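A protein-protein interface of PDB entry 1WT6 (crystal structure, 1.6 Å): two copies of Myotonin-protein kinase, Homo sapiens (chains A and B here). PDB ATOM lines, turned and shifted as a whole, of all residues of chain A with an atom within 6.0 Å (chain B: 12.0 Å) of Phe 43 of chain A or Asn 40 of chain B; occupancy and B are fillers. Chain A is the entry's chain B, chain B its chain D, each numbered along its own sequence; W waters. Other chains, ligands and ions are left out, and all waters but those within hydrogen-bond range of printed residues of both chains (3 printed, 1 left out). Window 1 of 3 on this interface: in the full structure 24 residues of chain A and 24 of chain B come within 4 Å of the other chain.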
ATOM      1  N   ILE A  36      29.755  12.357 -35.147  1.00  0.00           N
ATOM      2  CA  ILE A  36      28.584  13.013 -34.605  1.00  0.00           C
ATOM      3  C   ILE A  36      27.359  12.637 -35.452  1.00  0.00           C
ATOM      4  O   ILE A  36      26.333  12.243 -34.885  1.00  0.00           O
ATOM      5  CB  ILE A  36      28.815  14.530 -34.363  1.00  0.00           C
ATOM      6  CG1 ILE A  36      29.915  14.700 -33.313  1.00  0.00           C
ATOM      7  CG2 ILE A  36      27.574  15.151 -33.768  1.00  0.00           C
ATOM      8  CD1 ILE A  36      30.212  16.155 -32.927  1.00  0.00           C
ATOM      9  N   THR A  38      26.824   9.903 -37.350  1.00  0.00           N
ATOM     10  CA  THR A  38      26.516   8.504 -37.037  1.00  0.00           C
ATOM     11  C   THR A  38      25.833   8.375 -35.668  1.00  0.00           C
ATOM     12  O   THR A  38      24.786   7.725 -35.553  1.00  0.00           O
ATOM     13  CB  THR A  38      27.787   7.616 -37.056  1.00  0.00           C
ATOM     14  OG1 THR A  38      28.427   7.733 -38.334  1.00  0.00           O
ATOM     15  CG2 THR A  38      27.422   6.154 -36.802  1.00  0.00           C
ATOM     16  N   ASP A  39      26.402   9.017 -34.646  1.00  0.00           N
ATOM     17  CA  ASP A  39      25.828   8.953 -33.297  1.00  0.00           C
ATOM     18  C   ASP A  39      24.382   9.401 -33.365  1.00  0.00           C
ATOM     19  O   ASP A  39      23.500   8.722 -32.844  1.00  0.00           O
ATOM     20  CB  ASP A  39      26.634   9.764 -32.275  1.00  0.00           C
ATOM     21  CG  ASP A  39      27.941   9.063 -31.881  1.00  0.00           C
ATOM     22  OD1 ASP A  39      28.286   8.013 -32.503  1.00  0.00           O
ATOM     23  OD2 ASP A  39      28.647   9.571 -30.977  1.00  0.00           O
ATOM     24  N   ASN A  40      24.138  10.495 -34.071  1.00  0.00           N
ATOM     25  CA  ASN A  40      22.776  10.997 -34.263  1.00  0.00           C
ATOM     26  C   ASN A  40      21.780  10.076 -34.997  1.00  0.00           C
ATOM     27  O   ASN A  40      20.646   9.880 -34.527  1.00  0.00           O
ATOM     28  CB  ASN A  40      22.805  12.398 -34.872  1.00  0.00           C
ATOM     29  CG  ASN A  40      23.006  13.496 -33.818  1.00  0.00           C
ATOM     30  OD1 ASN A  40      23.236  13.239 -32.604  1.00  0.00           O
ATOM     31  ND2 ASN A  40      22.852  14.727 -34.267  1.00  0.00           N
ATOM     32  N   GLN A  41      22.187   9.504 -36.127  1.00  0.00           N
ATOM     33  CA  GLN A  41      21.401   8.428 -36.751  1.00  0.00           C
ATOM     34  C   GLN A  41      21.011   7.349 -35.703  1.00  0.00           C
ATOM     35  O   GLN A  41      19.845   6.882 -35.643  1.00  0.00           O
ATOM     36  CB  GLN A  41      22.207   7.796 -37.885  1.00  0.00           C
ATOM     37  CG  GLN A  41      22.621   8.747 -38.999  1.00  0.00           C
ATOM     38  CD  GLN A  41      21.555   8.930 -40.070  1.00  0.00           C
ATOM     39  OE1 GLN A  41      21.785   9.609 -41.078  1.00  0.00           O
ATOM     40  NE2 GLN A  41      20.384   8.324 -39.860  1.00  0.00           N
ATOM     41  N   ASN A  42      21.978   6.950 -34.879  1.00  0.00           N
ATOM     42  CA  ASN A  42      21.706   5.945 -33.846  1.00  0.00           C
ATOM     43  C   ASN A  42      20.700   6.453 -32.809  1.00  0.00           C
ATOM     44  O   ASN A  42      19.812   5.718 -32.374  1.00  0.00           O
ATOM     45  CB  ASN A  42      22.993   5.487 -33.171  1.00  0.00           C
ATOM     46  CG  ASN A  42      23.889   4.682 -34.108  1.00  0.00           C
ATOM     47  OD1 ASN A  42      23.429   4.115 -35.119  1.00  0.00           O
ATOM     48  ND2 ASN A  42      25.186   4.651 -33.790  1.00  0.00           N
ATOM     49  N   PHE A  43      20.866   7.691 -32.370  1.00  0.00           N
ATOM     50  CA  PHE A  43      19.926   8.228 -31.408  1.00  0.00           C
ATOM     51  C   PHE A  43      18.519   8.133 -31.962  1.00  0.00           C
ATOM     52  O   PHE A  43      17.614   7.707 -31.210  1.00  0.00           O
ATOM     53  CB  PHE A  43      20.252   9.658 -30.969  1.00  0.00           C
ATOM     54  CG  PHE A  43      21.556   9.779 -30.210  1.00  0.00           C
ATOM     55  CD1 PHE A  43      22.321  10.931 -30.330  1.00  0.00           C
ATOM     56  CD2 PHE A  43      22.027   8.753 -29.394  1.00  0.00           C
ATOM     57  CE1 PHE A  43      23.502  11.058 -29.625  1.00  0.00           C
ATOM     58  CE2 PHE A  43      23.237   8.881 -28.700  1.00  0.00           C
ATOM     59  CZ  PHE A  43      23.977  10.045 -28.847  1.00  0.00           C
ATOM     60  N   ALA A  44      18.327   8.531 -33.234  1.00  0.00           N
ATOM     61  CA  ALA A  44      16.984   8.503 -33.855  1.00  0.00           C
ATOM     62  C   ALA A  44      16.347   7.073 -33.762  1.00  0.00           C
ATOM     63  O   ALA A  44      15.198   6.893 -33.353  1.00  0.00           O
ATOM     64  CB  ALA A  44      17.026   8.966 -35.323  1.00  0.00           C
ATOM     65  N   SER A  45      17.120   6.067 -34.112  1.00  0.00           N
ATOM     66  CA  SER A  45      16.648   4.676 -34.045  1.00  0.00           C
ATOM     67  C   SER A  45      16.381   4.222 -32.605  1.00  0.00           C
ATOM     68  O   SER A  45      15.321   3.586 -32.324  1.00  0.00           O
ATOM     69  CB  SER A  45      17.691   3.748 -34.679  1.00  0.00           C
ATOM     70  OG  SER A  45      17.589   3.883 -36.087  1.00  0.00           O
ATOM     71  N   GLN A  46      17.285   4.588 -31.680  1.00  0.00           N
ATOM     72  CA  GLN A  46      17.131   4.185 -30.281  1.00  0.00           C
ATOM     73  C   GLN A  46      15.881   4.806 -29.673  1.00  0.00           C
ATOM     74  O   GLN A  46      15.162   4.150 -28.904  1.00  0.00           O
ATOM     75  CB  GLN A  46      18.357   4.511 -29.426  1.00  0.00           C
ATOM     76  CG  GLN A  46      19.584   3.714 -29.847  1.00  0.00           C
ATOM     77  CD  GLN A  46      20.878   4.380 -29.404  1.00  0.00           C
ATOM     78  OE1 GLN A  46      20.976   4.890 -28.284  1.00  0.00           O
ATOM     79  NE2 GLN A  46      21.882   4.380 -30.291  1.00  0.00           N
ATOM     80  N   LEU A  47      15.627   6.082 -29.967  1.00  0.00           N
ATOM     81  CA  LEU A  47      14.425   6.724 -29.475  1.00  0.00           C
ATOM     82  C   LEU A  47      13.163   6.053 -30.039  1.00  0.00           C
ATOM     83  O   LEU A  47      12.173   5.801 -29.312  1.00  0.00           O
ATOM     84  CB  LEU A  47      14.439   8.213 -29.830  1.00  0.00           C
ATOM     85  CG  LEU A  47      15.467   9.049 -29.042  1.00  0.00           C
ATOM     86  CD1 LEU A  47      15.565  10.458 -29.647  1.00  0.00           C
ATOM     87  CD2 LEU A  47      15.128   9.128 -27.534  1.00  0.00           C
ATOM     88  N   ARG A  48      13.174   5.735 -31.338  1.00  0.00           N
ATOM     89  CA  ARG A  48      12.005   5.054 -31.913  1.00  0.00           C
ATOM     90  C   ARG A  48      11.754   3.716 -31.193  1.00  0.00           C
ATOM     91  O   ARG A  48      10.618   3.339 -30.872  1.00  0.00           O
ATOM     92  CB  ARG A  48      12.190   4.767 -33.431  1.00  0.00           C
ATOM     93  CG  ARG A  48      11.795   5.917 -34.362  1.00  0.00           C
ATOM     94  CD  ARG A  48      11.786   5.454 -35.862  1.00  0.00           C
ATOM     95  NE  ARG A  48      13.131   5.233 -36.364  1.00  0.00           N
ATOM     96  CZ  ARG A  48      13.920   6.182 -36.855  1.00  0.00           C
ATOM     97  NH1 ARG A  48      13.509   7.451 -36.926  1.00  0.00           N
ATOM     98  NH2 ARG A  48      15.131   5.852 -37.278  1.00  0.00           N
ATOM     99  N   ARG B  31      35.021  24.722 -32.154  1.00  0.00           N
ATOM    100  CA  ARG B  31      34.479  24.914 -30.796  1.00  0.00           C
ATOM    101  C   ARG B  31      33.078  24.361 -30.705  1.00  0.00           C
ATOM    102  O   ARG B  31      32.703  23.726 -29.689  1.00  0.00           O
ATOM    103  CB  ARG B  31      34.482  26.405 -30.417  1.00  0.00           C
ATOM    104  CG  ARG B  31      35.869  26.896 -30.284  1.00  0.00           C
ATOM    105  CD  ARG B  31      35.905  28.312 -29.894  1.00  0.00           C
ATOM    106  NE  ARG B  31      37.249  28.745 -30.242  1.00  0.00           N
ATOM    107  CZ  ARG B  31      37.617  29.574 -31.209  1.00  0.00           C
ATOM    108  NH1 ARG B  31      36.748  30.381 -31.857  1.00  0.00           N
ATOM    109  NH2 ARG B  31      38.924  29.706 -31.390  1.00  0.00           N
ATOM    110  N   GLU B  32      32.276  24.651 -31.723  1.00  0.00           N
ATOM    111  CA  GLU B  32      30.885  24.196 -31.723  1.00  0.00           C
ATOM    112  C   GLU B  32      30.870  22.682 -31.723  1.00  0.00           C
ATOM    113  O   GLU B  32      30.135  22.079 -30.925  1.00  0.00           O
ATOM    114  CB  GLU B  32      30.180  24.663 -32.956  1.00  0.00           C
ATOM    115  CG  GLU B  32      29.798  26.109 -32.950  1.00  0.00           C
ATOM    116  CD  GLU B  32      29.012  26.414 -34.176  1.00  0.00           C
ATOM    117  OE1 GLU B  32      27.989  25.729 -34.383  1.00  0.00           O
ATOM    118  OE2 GLU B  32      29.427  27.298 -34.950  1.00  0.00           O
ATOM    119  N   MET B  33      31.730  22.067 -32.527  1.00  0.00           N
ATOM    120  CA  MET B  33      31.768  20.600 -32.593  1.00  0.00           C
ATOM    121  C   MET B  33      32.111  20.023 -31.206  1.00  0.00           C
ATOM    122  O   MET B  33      31.495  19.030 -30.762  1.00  0.00           O
ATOM    123  CB  MET B  33      32.779  20.116 -33.635  1.00  0.00           C
ATOM    124  CG  MET B  33      33.101  18.628 -33.581  1.00  0.00           C
ATOM    125  SD  MET B  33      34.244  18.168 -32.252  1.00  0.00           S
ATOM    126  CE  MET B  33      35.675  19.232 -32.634  1.00  0.00           C
ATOM    127  N   GLU B  34      33.121  20.610 -30.566  1.00  0.00           N
ATOM    128  CA  GLU B  34      33.525  20.216 -29.202  1.00  0.00           C
ATOM    129  C   GLU B  34      32.362  20.222 -28.206  1.00  0.00           C
ATOM    130  O   GLU B  34      32.215  19.280 -27.405  1.00  0.00           O
ATOM    131  CB  GLU B  34      34.652  21.109 -28.691  1.00  0.00           C
ATOM    132  CG  GLU B  34      36.012  20.707 -29.193  1.00  0.00           C
ATOM    133  CD  GLU B  34      37.111  21.345 -28.371  1.00  0.00           C
ATOM    134  OE1 GLU B  34      37.236  22.607 -28.393  1.00  0.00           O
ATOM    135  OE2 GLU B  34      37.837  20.578 -27.696  1.00  0.00           O
ATOM    136  N   ALA B  35      31.546  21.278 -28.282  1.00  0.00           N
ATOM    137  CA  ALA B  35      30.414  21.498 -27.392  1.00  0.00           C
ATOM    138  C   ALA B  35      29.379  20.402 -27.658  1.00  0.00           C
ATOM    139  O   ALA B  35      28.910  19.750 -26.696  1.00  0.00           O
ATOM    140  CB  ALA B  35      29.816  22.874 -27.636  1.00  0.00           C
ATOM    141  N   ILE B  36      29.111  20.137 -28.937  1.00  0.00           N
ATOM    142  CA  ILE B  36      28.189  19.058 -29.322  1.00  0.00           C
ATOM    143  C   ILE B  36      28.691  17.663 -28.982  1.00  0.00           C
ATOM    144  O   ILE B  36      27.897  16.842 -28.522  1.00  0.00           O
ATOM    145  CB  ILE B  36      27.754  19.158 -30.783  1.00  0.00           C
ATOM    146  CG1 ILE B  36      26.826  20.396 -30.932  1.00  0.00           C
ATOM    147  CG2 ILE B  36      27.120  17.853 -31.364  1.00  0.00           C
ATOM    148  CD1 ILE B  36      26.714  20.887 -32.328  1.00  0.00           C
ATOM    149  N   ARG B  37      29.971  17.374 -29.181  1.00  0.00           N
ATOM    150  CA  ARG B  37      30.503  16.047 -28.796  1.00  0.00           C
ATOM    151  C   ARG B  37      30.154  15.820 -27.298  1.00  0.00           C
ATOM    152  O   ARG B  37      29.510  14.793 -26.938  1.00  0.00           O
ATOM    153  CB  ARG B  37      32.005  16.047 -29.089  1.00  0.00           C
ATOM    154  CG  ARG B  37      32.783  14.708 -28.988  1.00  0.00           C
ATOM    155  CD  ARG B  37      34.233  14.974 -29.477  1.00  0.00           C
ATOM    156  NE  ARG B  37      34.948  15.882 -28.571  1.00  0.00           N
ATOM    157  CZ  ARG B  37      36.162  16.405 -28.777  1.00  0.00           C
ATOM    158  NH1 ARG B  37      36.852  16.134 -29.883  1.00  0.00           N
ATOM    159  NH2 ARG B  37      36.701  17.203 -27.861  1.00  0.00           N
ATOM    160  N   THR B  38      30.477  16.808 -26.460  1.00  0.00           N
ATOM    161  CA  THR B  38      30.204  16.693 -25.010  1.00  0.00           C
ATOM    162  C   THR B  38      28.708  16.496 -24.791  1.00  0.00           C
ATOM    163  O   THR B  38      28.274  15.601 -24.059  1.00  0.00           O
ATOM    164  CB  THR B  38      30.701  17.925 -24.246  1.00  0.00           C
ATOM    165  OG1 THR B  38      32.127  17.968 -24.338  1.00  0.00           O
ATOM    166  CG2 THR B  38      30.395  17.774 -22.753  1.00  0.00           C
ATOM    167  N   ASP B  39      27.925  17.417 -25.343  1.00  0.00           N
ATOM    168  CA  ASP B  39      26.451  17.309 -25.288  1.00  0.00           C
ATOM    169  C   ASP B  39      25.919  15.911 -25.663  1.00  0.00           C
ATOM    170  O   ASP B  39      25.026  15.374 -24.955  1.00  0.00           O
ATOM    171  CB  ASP B  39      25.762  18.316 -26.196  1.00  0.00           C
ATOM    172  CG  ASP B  39      25.898  19.775 -25.697  1.00  0.00           C
ATOM    173  OD1 ASP B  39      26.386  20.005 -24.561  1.00  0.00           O
ATOM    174  OD2 ASP B  39      25.533  20.687 -26.482  1.00  0.00           O
ATOM    175  N   ASN B  40      26.375  15.384 -26.806  1.00  0.00           N
ATOM    176  CA  ASN B  40      25.846  14.104 -27.312  1.00  0.00           C
ATOM    177  C   ASN B  40      26.160  13.026 -26.305  1.00  0.00           C
ATOM    178  O   ASN B  40      25.375  12.078 -26.165  1.00  0.00           O
ATOM    179  CB  ASN B  40      26.409  13.728 -28.692  1.00  0.00           C
ATOM    180  CG  ASN B  40      25.594  14.296 -29.794  1.00  0.00           C
ATOM    181  OD1 ASN B  40      24.694  15.123 -29.556  1.00  0.00           O
ATOM    182  ND2 ASN B  40      25.861  13.857 -31.015  1.00  0.00           N
ATOM    183  N   GLN B  41      27.302  13.145 -25.635  1.00  0.00           N
ATOM    184  CA  GLN B  41      27.653  12.122 -24.619  1.00  0.00           C
ATOM    185  C   GLN B  41      26.718  12.130 -23.415  1.00  0.00           C
ATOM    186  O   GLN B  41      26.248  11.081 -22.922  1.00  0.00           O
ATOM    187  CB  GLN B  41      29.120  12.162 -24.219  1.00  0.00           C
ATOM    188  CG  GLN B  41      30.083  11.544 -25.298  1.00  0.00           C
ATOM    189  CD  GLN B  41      29.594  10.202 -25.911  1.00  0.00           C
ATOM    190  OE1 GLN B  41      29.372  10.110 -27.135  1.00  0.00           O
ATOM    191  NE2 GLN B  41      29.443   9.165 -25.071  1.00  0.00           N
ATOM    192  N   ASN B  42      26.433  13.324 -22.932  1.00  0.00           N
ATOM    193  CA  ASN B  42      25.500  13.505 -21.835  1.00  0.00           C
ATOM    194  C   ASN B  42      24.126  13.060 -22.274  1.00  0.00           C
ATOM    195  O   ASN B  42      23.424  12.363 -21.551  1.00  0.00           O
ATOM    196  CB  ASN B  42      25.543  14.970 -21.406  1.00  0.00           C
ATOM    197  CG  ASN B  42      26.844  15.296 -20.670  1.00  0.00           C
ATOM    198  OD1 ASN B  42      27.416  14.428 -19.979  1.00  0.00           O
ATOM    199  ND2 ASN B  42      27.320  16.543 -20.795  1.00  0.00           N
ATOM    200  N   PHE B  43      23.717  13.409 -23.470  1.00  0.00           N
ATOM    201  CA  PHE B  43      22.482  12.871 -23.996  1.00  0.00           C
ATOM    202  C   PHE B  43      22.367  11.310 -24.059  1.00  0.00           C
ATOM    203  O   PHE B  43      21.373  10.714 -23.585  1.00  0.00           O
ATOM    204  CB  PHE B  43      22.234  13.365 -25.395  1.00  0.00           C
ATOM    205  CG  PHE B  43      20.916  12.923 -25.932  1.00  0.00           C
ATOM    206  CD1 PHE B  43      19.708  13.604 -25.541  1.00  0.00           C
ATOM    207  CD2 PHE B  43      20.848  11.825 -26.779  1.00  0.00           C
ATOM    208  CE1 PHE B  43      18.481  13.162 -26.019  1.00  0.00           C
ATOM    209  CE2 PHE B  43      19.597  11.381 -27.297  1.00  0.00           C
ATOM    210  CZ  PHE B  43      18.407  12.058 -26.903  1.00  0.00           C
ATOM    211  N   ALA B  44      23.368  10.664 -24.662  1.00  0.00           N
ATOM    212  CA  ALA B  44      23.357   9.208 -24.741  1.00  0.00           C
ATOM    213  C   ALA B  44      23.243   8.608 -23.319  1.00  0.00           C
ATOM    214  O   ALA B  44      22.564   7.599 -23.135  1.00  0.00           O
ATOM    215  CB  ALA B  44      24.710   8.732 -25.410  1.00  0.00           C
ATOM    216  N   SER B  45      23.881   9.212 -22.322  1.00  0.00           N
ATOM    217  CA  SER B  45      23.840   8.733 -20.922  1.00  0.00           C
ATOM    218  C   SER B  45      22.375   8.875 -20.448  1.00  0.00           C
ATOM    219  O   SER B  45      21.840   7.980 -19.834  1.00  0.00           O
ATOM    220  CB  SER B  45      24.681   9.586 -19.987  1.00  0.00           C
ATOM    221  OG  SER B  45      26.027   9.649 -20.424  1.00  0.00           O
ATOM    222  N   GLN B  46      21.718  10.001 -20.739  1.00  0.00           N
ATOM    223  CA  GLN B  46      20.322  10.120 -20.371  1.00  0.00           C
ATOM    224  C   GLN B  46      19.408   9.115 -21.065  1.00  0.00           C
ATOM    225  O   GLN B  46      18.487   8.523 -20.448  1.00  0.00           O
ATOM    226  CB  GLN B  46      19.853  11.553 -20.714  1.00  0.00           C
ATOM    227  CG  GLN B  46      20.446  12.568 -19.785  1.00  0.00           C
ATOM    228  CD  GLN B  46      20.225  14.008 -20.274  1.00  0.00           C
ATOM    229  OE1 GLN B  46      19.708  14.237 -21.368  1.00  0.00           O
ATOM    230  NE2 GLN B  46      20.636  14.974 -19.460  1.00  0.00           N
ATOM    231  N   LEU B  47      19.657   8.828 -22.329  1.00  0.00           N
ATOM    232  CA  LEU B  47      18.902   7.869 -23.046  1.00  0.00           C
ATOM    233  C   LEU B  47      19.043   6.435 -22.433  1.00  0.00           C
ATOM    234  O   LEU B  47      18.057   5.742 -22.187  1.00  0.00           O
ATOM    235  CB  LEU B  47      19.424   7.874 -24.458  1.00  0.00           C
ATOM    236  CG  LEU B  47      18.739   6.904 -25.345  1.00  0.00           C
ATOM    237  CD1 LEU B  47      17.140   6.897 -25.243  1.00  0.00           C
ATOM    238  CD2 LEU B  47      19.181   7.219 -26.732  1.00  0.00           C
ATOM    239  N   ARG B  48      20.278   6.078 -22.101  1.00  0.00           N
ATOM    240  CA  ARG B  48      20.518   4.739 -21.458  1.00  0.00           C
ATOM    241  C   ARG B  48      19.781   4.659 -20.107  1.00  0.00           C
ATOM    242  O   ARG B  48      19.194   3.637 -19.760  1.00  0.00           O
ATOM    243  CB  ARG B  48      22.027   4.503 -21.291  1.00  0.00           C
ATOM    244  CG  ARG B  48      22.690   4.233 -22.616  1.00  0.00           C
ATOM    245  CD  ARG B  48      24.142   3.815 -22.434  1.00  0.00           C
ATOM    246  NE  ARG B  48      24.997   4.783 -21.796  1.00  0.00           N
ATOM    247  CZ  ARG B  48      25.762   5.663 -22.439  1.00  0.00           C
ATOM    248  NH1 ARG B  48      25.644   5.839 -23.741  1.00  0.00           N
ATOM    249  NH2 ARG B  48      26.574   6.452 -21.735  1.00  0.00           N
ATOM    250  N   GLU B  49      19.787   5.772 -19.335  1.00  0.00           N
ATOM    251  CA  GLU B  49      19.007   5.775 -18.087  1.00  0.00           C
ATOM    252  C   GLU B  49      17.511   5.519 -18.314  1.00  0.00           C
ATOM    253  O   GLU B  49      16.853   4.761 -17.576  1.00  0.00           O
ATOM    254  CB  GLU B  49      19.231   6.998 -17.270  1.00  0.00           C
ATOM    255  CG  GLU B  49      18.843   6.703 -15.750  1.00  0.00           C
ATOM    256  CD  GLU B  49      18.941   5.153 -15.212  1.00  0.00           C
ATOM    257  OE1 GLU B  49      20.071   4.488 -15.116  1.00  0.00           O
ATOM    258  OE2 GLU B  49      17.840   4.590 -14.814  1.00  0.00           O
ATOM    259  N   ALA B  50      16.928   6.188 -19.329  1.00  0.00           N
ATOM    260  CA  ALA B  50      15.570   5.873 -19.703  1.00  0.00           C
ATOM    261  C   ALA B  50      15.283   4.452 -20.146  1.00  0.00           C
ATOM    262  O   ALA B  50      14.257   3.853 -19.720  1.00  0.00           O
ATOM    263  CB  ALA B  50      15.011   6.870 -20.759  1.00  0.00           C
ATOM    264  N   GLU B  51      16.222   3.843 -20.887  1.00  0.00           N
ATOM    265  CA  GLU B  51      16.122   2.455 -21.293  1.00  0.00           C
ATOM    266  C   GLU B  51      16.126   1.593 -20.012  1.00  0.00           C
ATOM    267  O   GLU B  51      15.354   0.651 -19.867  1.00  0.00           O
ATOM    268  CB  GLU B  51      17.288   2.112 -22.242  1.00  0.00           C
ATOM    269  CG  GLU B  51      17.049   2.764 -23.625  1.00  0.00           C
ATOM    270  CD  GLU B  51      18.279   2.750 -24.564  1.00  0.00           C
ATOM    271  OE1 GLU B  51      19.457   2.804 -24.110  1.00  0.00           O
ATOM    272  OE2 GLU B  51      18.062   2.782 -25.795  1.00  0.00           O
HETATM  273  O   HOH W   1      28.175  12.070 -31.204  1.00  0.00           O
HETATM  274  O   HOH W   2      16.232   2.123 -27.443  1.00  0.00           O
HETATM  275  O   HOH W   3      21.007   3.637 -25.828  1.00  0.00           O
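O of Asn 42 of chain A sits at hydrogen-bond distance from NE2 of Gln 46 of chain A (3.2 Å). The side-chain carboxylate (OE2) of Glu 34 of chain B is in salt-bridge range of the guanidinium group (NH2) of Arg 37 of chain B. The backbone carbonyl oxygen (O) of Gln 41 of chain B is in hydrogen-bond range of the side-chain hydroxyl (OG) of Ser 45 of chain B, at 2.9 Å.
Asp 39 of chain A touches Gln 41 of chain B, but with the chains exchanged Gln 41 of chain A does not touch Asp 39 of chain B (12.8 Å). Phe 43 of chain B touches its own counterpart, Phe 43 of chain A. Phe 43 of chain A touches Ala 44 of chain B, but with the chains exchanged Ala 44 of chain A does not touch Phe 43 of chain B (6.7 Å). Leu 47 of chain A touches its own counterpart, Leu 47 of chain B. Of the 11 pairs that touch across the chains among the printed residues, 4 have their exchanged pair printed and touching as well.
Water W3 lies within hydrogen-bond range of the side-chain carboxylate of Glu 51 of chain B (2.5 Å) and the side-chain amide oxygen of Gln 46 of chain A (2.8 Å). Water W2 lies within hydrogen-bond range of OE2 of Glu 51 of chain B (2.5 Å) and O of Gln 46 of chain A (2.7 Å). Water W1 bridges OD2 of Asp 39 of chain A and ND2 of Asn 40 of chain B.
Among the printed residues, pairs that only touch across the chains: Ile 36 of chain A with Met 33 of chain B (3.8 Å), Ile 36 of chain A with Ile 36 of chain B (3.6 Å), Ile 36 of chain A with Arg 37 of chain B (3.9 Å), Ile 36 of chain A with Asn 40 of chain B (3.5 Å), Asp 39 of chain A with Gln 41 of chain B (3.9 Å), Phe 43 of chain A with Asn 40 of chain B (3.6 Å), Phe 43 of chain A with Phe 43 of chain B (3.9 Å), Phe 43 of chain A with Ala 44 of chain B (3.6 Å), Gln 46 of chain A with Leu 47 of chain B (3.3 Å) and Leu 47 of chain A with Leu 47 of chain B (3.8 Å).
ND2 of Asn 40 of chain B is in hydrogen-bond range of OD1 of Asn 40 of chain A.
Printed residues of chain A that touch a printed residue of chain B: Ile 36, Asp 39, Asn 40, Phe 43, Gln 46 and Leu 47. Hydrophobic or aromatic side chains of chain A within 4 Å of the printed part of chain B: Ile 36, Phe 43 and Leu 47. Along chain A the printed residues that touch a printed residue of chain B span positions 36 to 47.
Of chain B, only Asn 40 (3.6 Å), Phe 43 (3.9 Å) and Ala 44 (3.6 Å) come within 4 Å of Phe 43 of chain A. Asn 40 of chain B touches just these residues of chain A: Ile 36, Asn 40 and Phe 43. Ile 36 of chain A touches just these residues of chain B: Met 33, Ile 36, Arg 37 and Asn 40. Asn 40 of chain A touches just one residue of chain B: Asn 40 (3.1 Å). No residue of chain B comes within 4 Å of Asn 42 of chain A. No residue of chain B comes within 4 Å of Ser 45 of chain A. Of the printed residues of chain B, Gln 46 of chain A touches Leu 47. Of the printed residues of chain A, Ala 44 of chain B touches Phe 43 (3.6 Å). Of the printed residues of chain A, Phe 43 of chain B touches Phe 43. Of the printed residues of chain A, Gln 41 of chain B touches Asp 39 (3.9 Å). Printed residues of chain A within 4 Å of Arg 37 of chain B: Ile 36 (3.9 Å). Of the printed residues of chain B, Leu 47 of chain A touches Leu 47. Gln 46 of chain B touches none of the printed residues of chain A. The nearest residue of chain B that does not touch Phe 43 of chain A is Leu 47 of chain B (4.2 Å). The nearest printed residue of chain A that does not touch Ile 36 of chain B is Asn 40 of chain A (6.0 Å).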
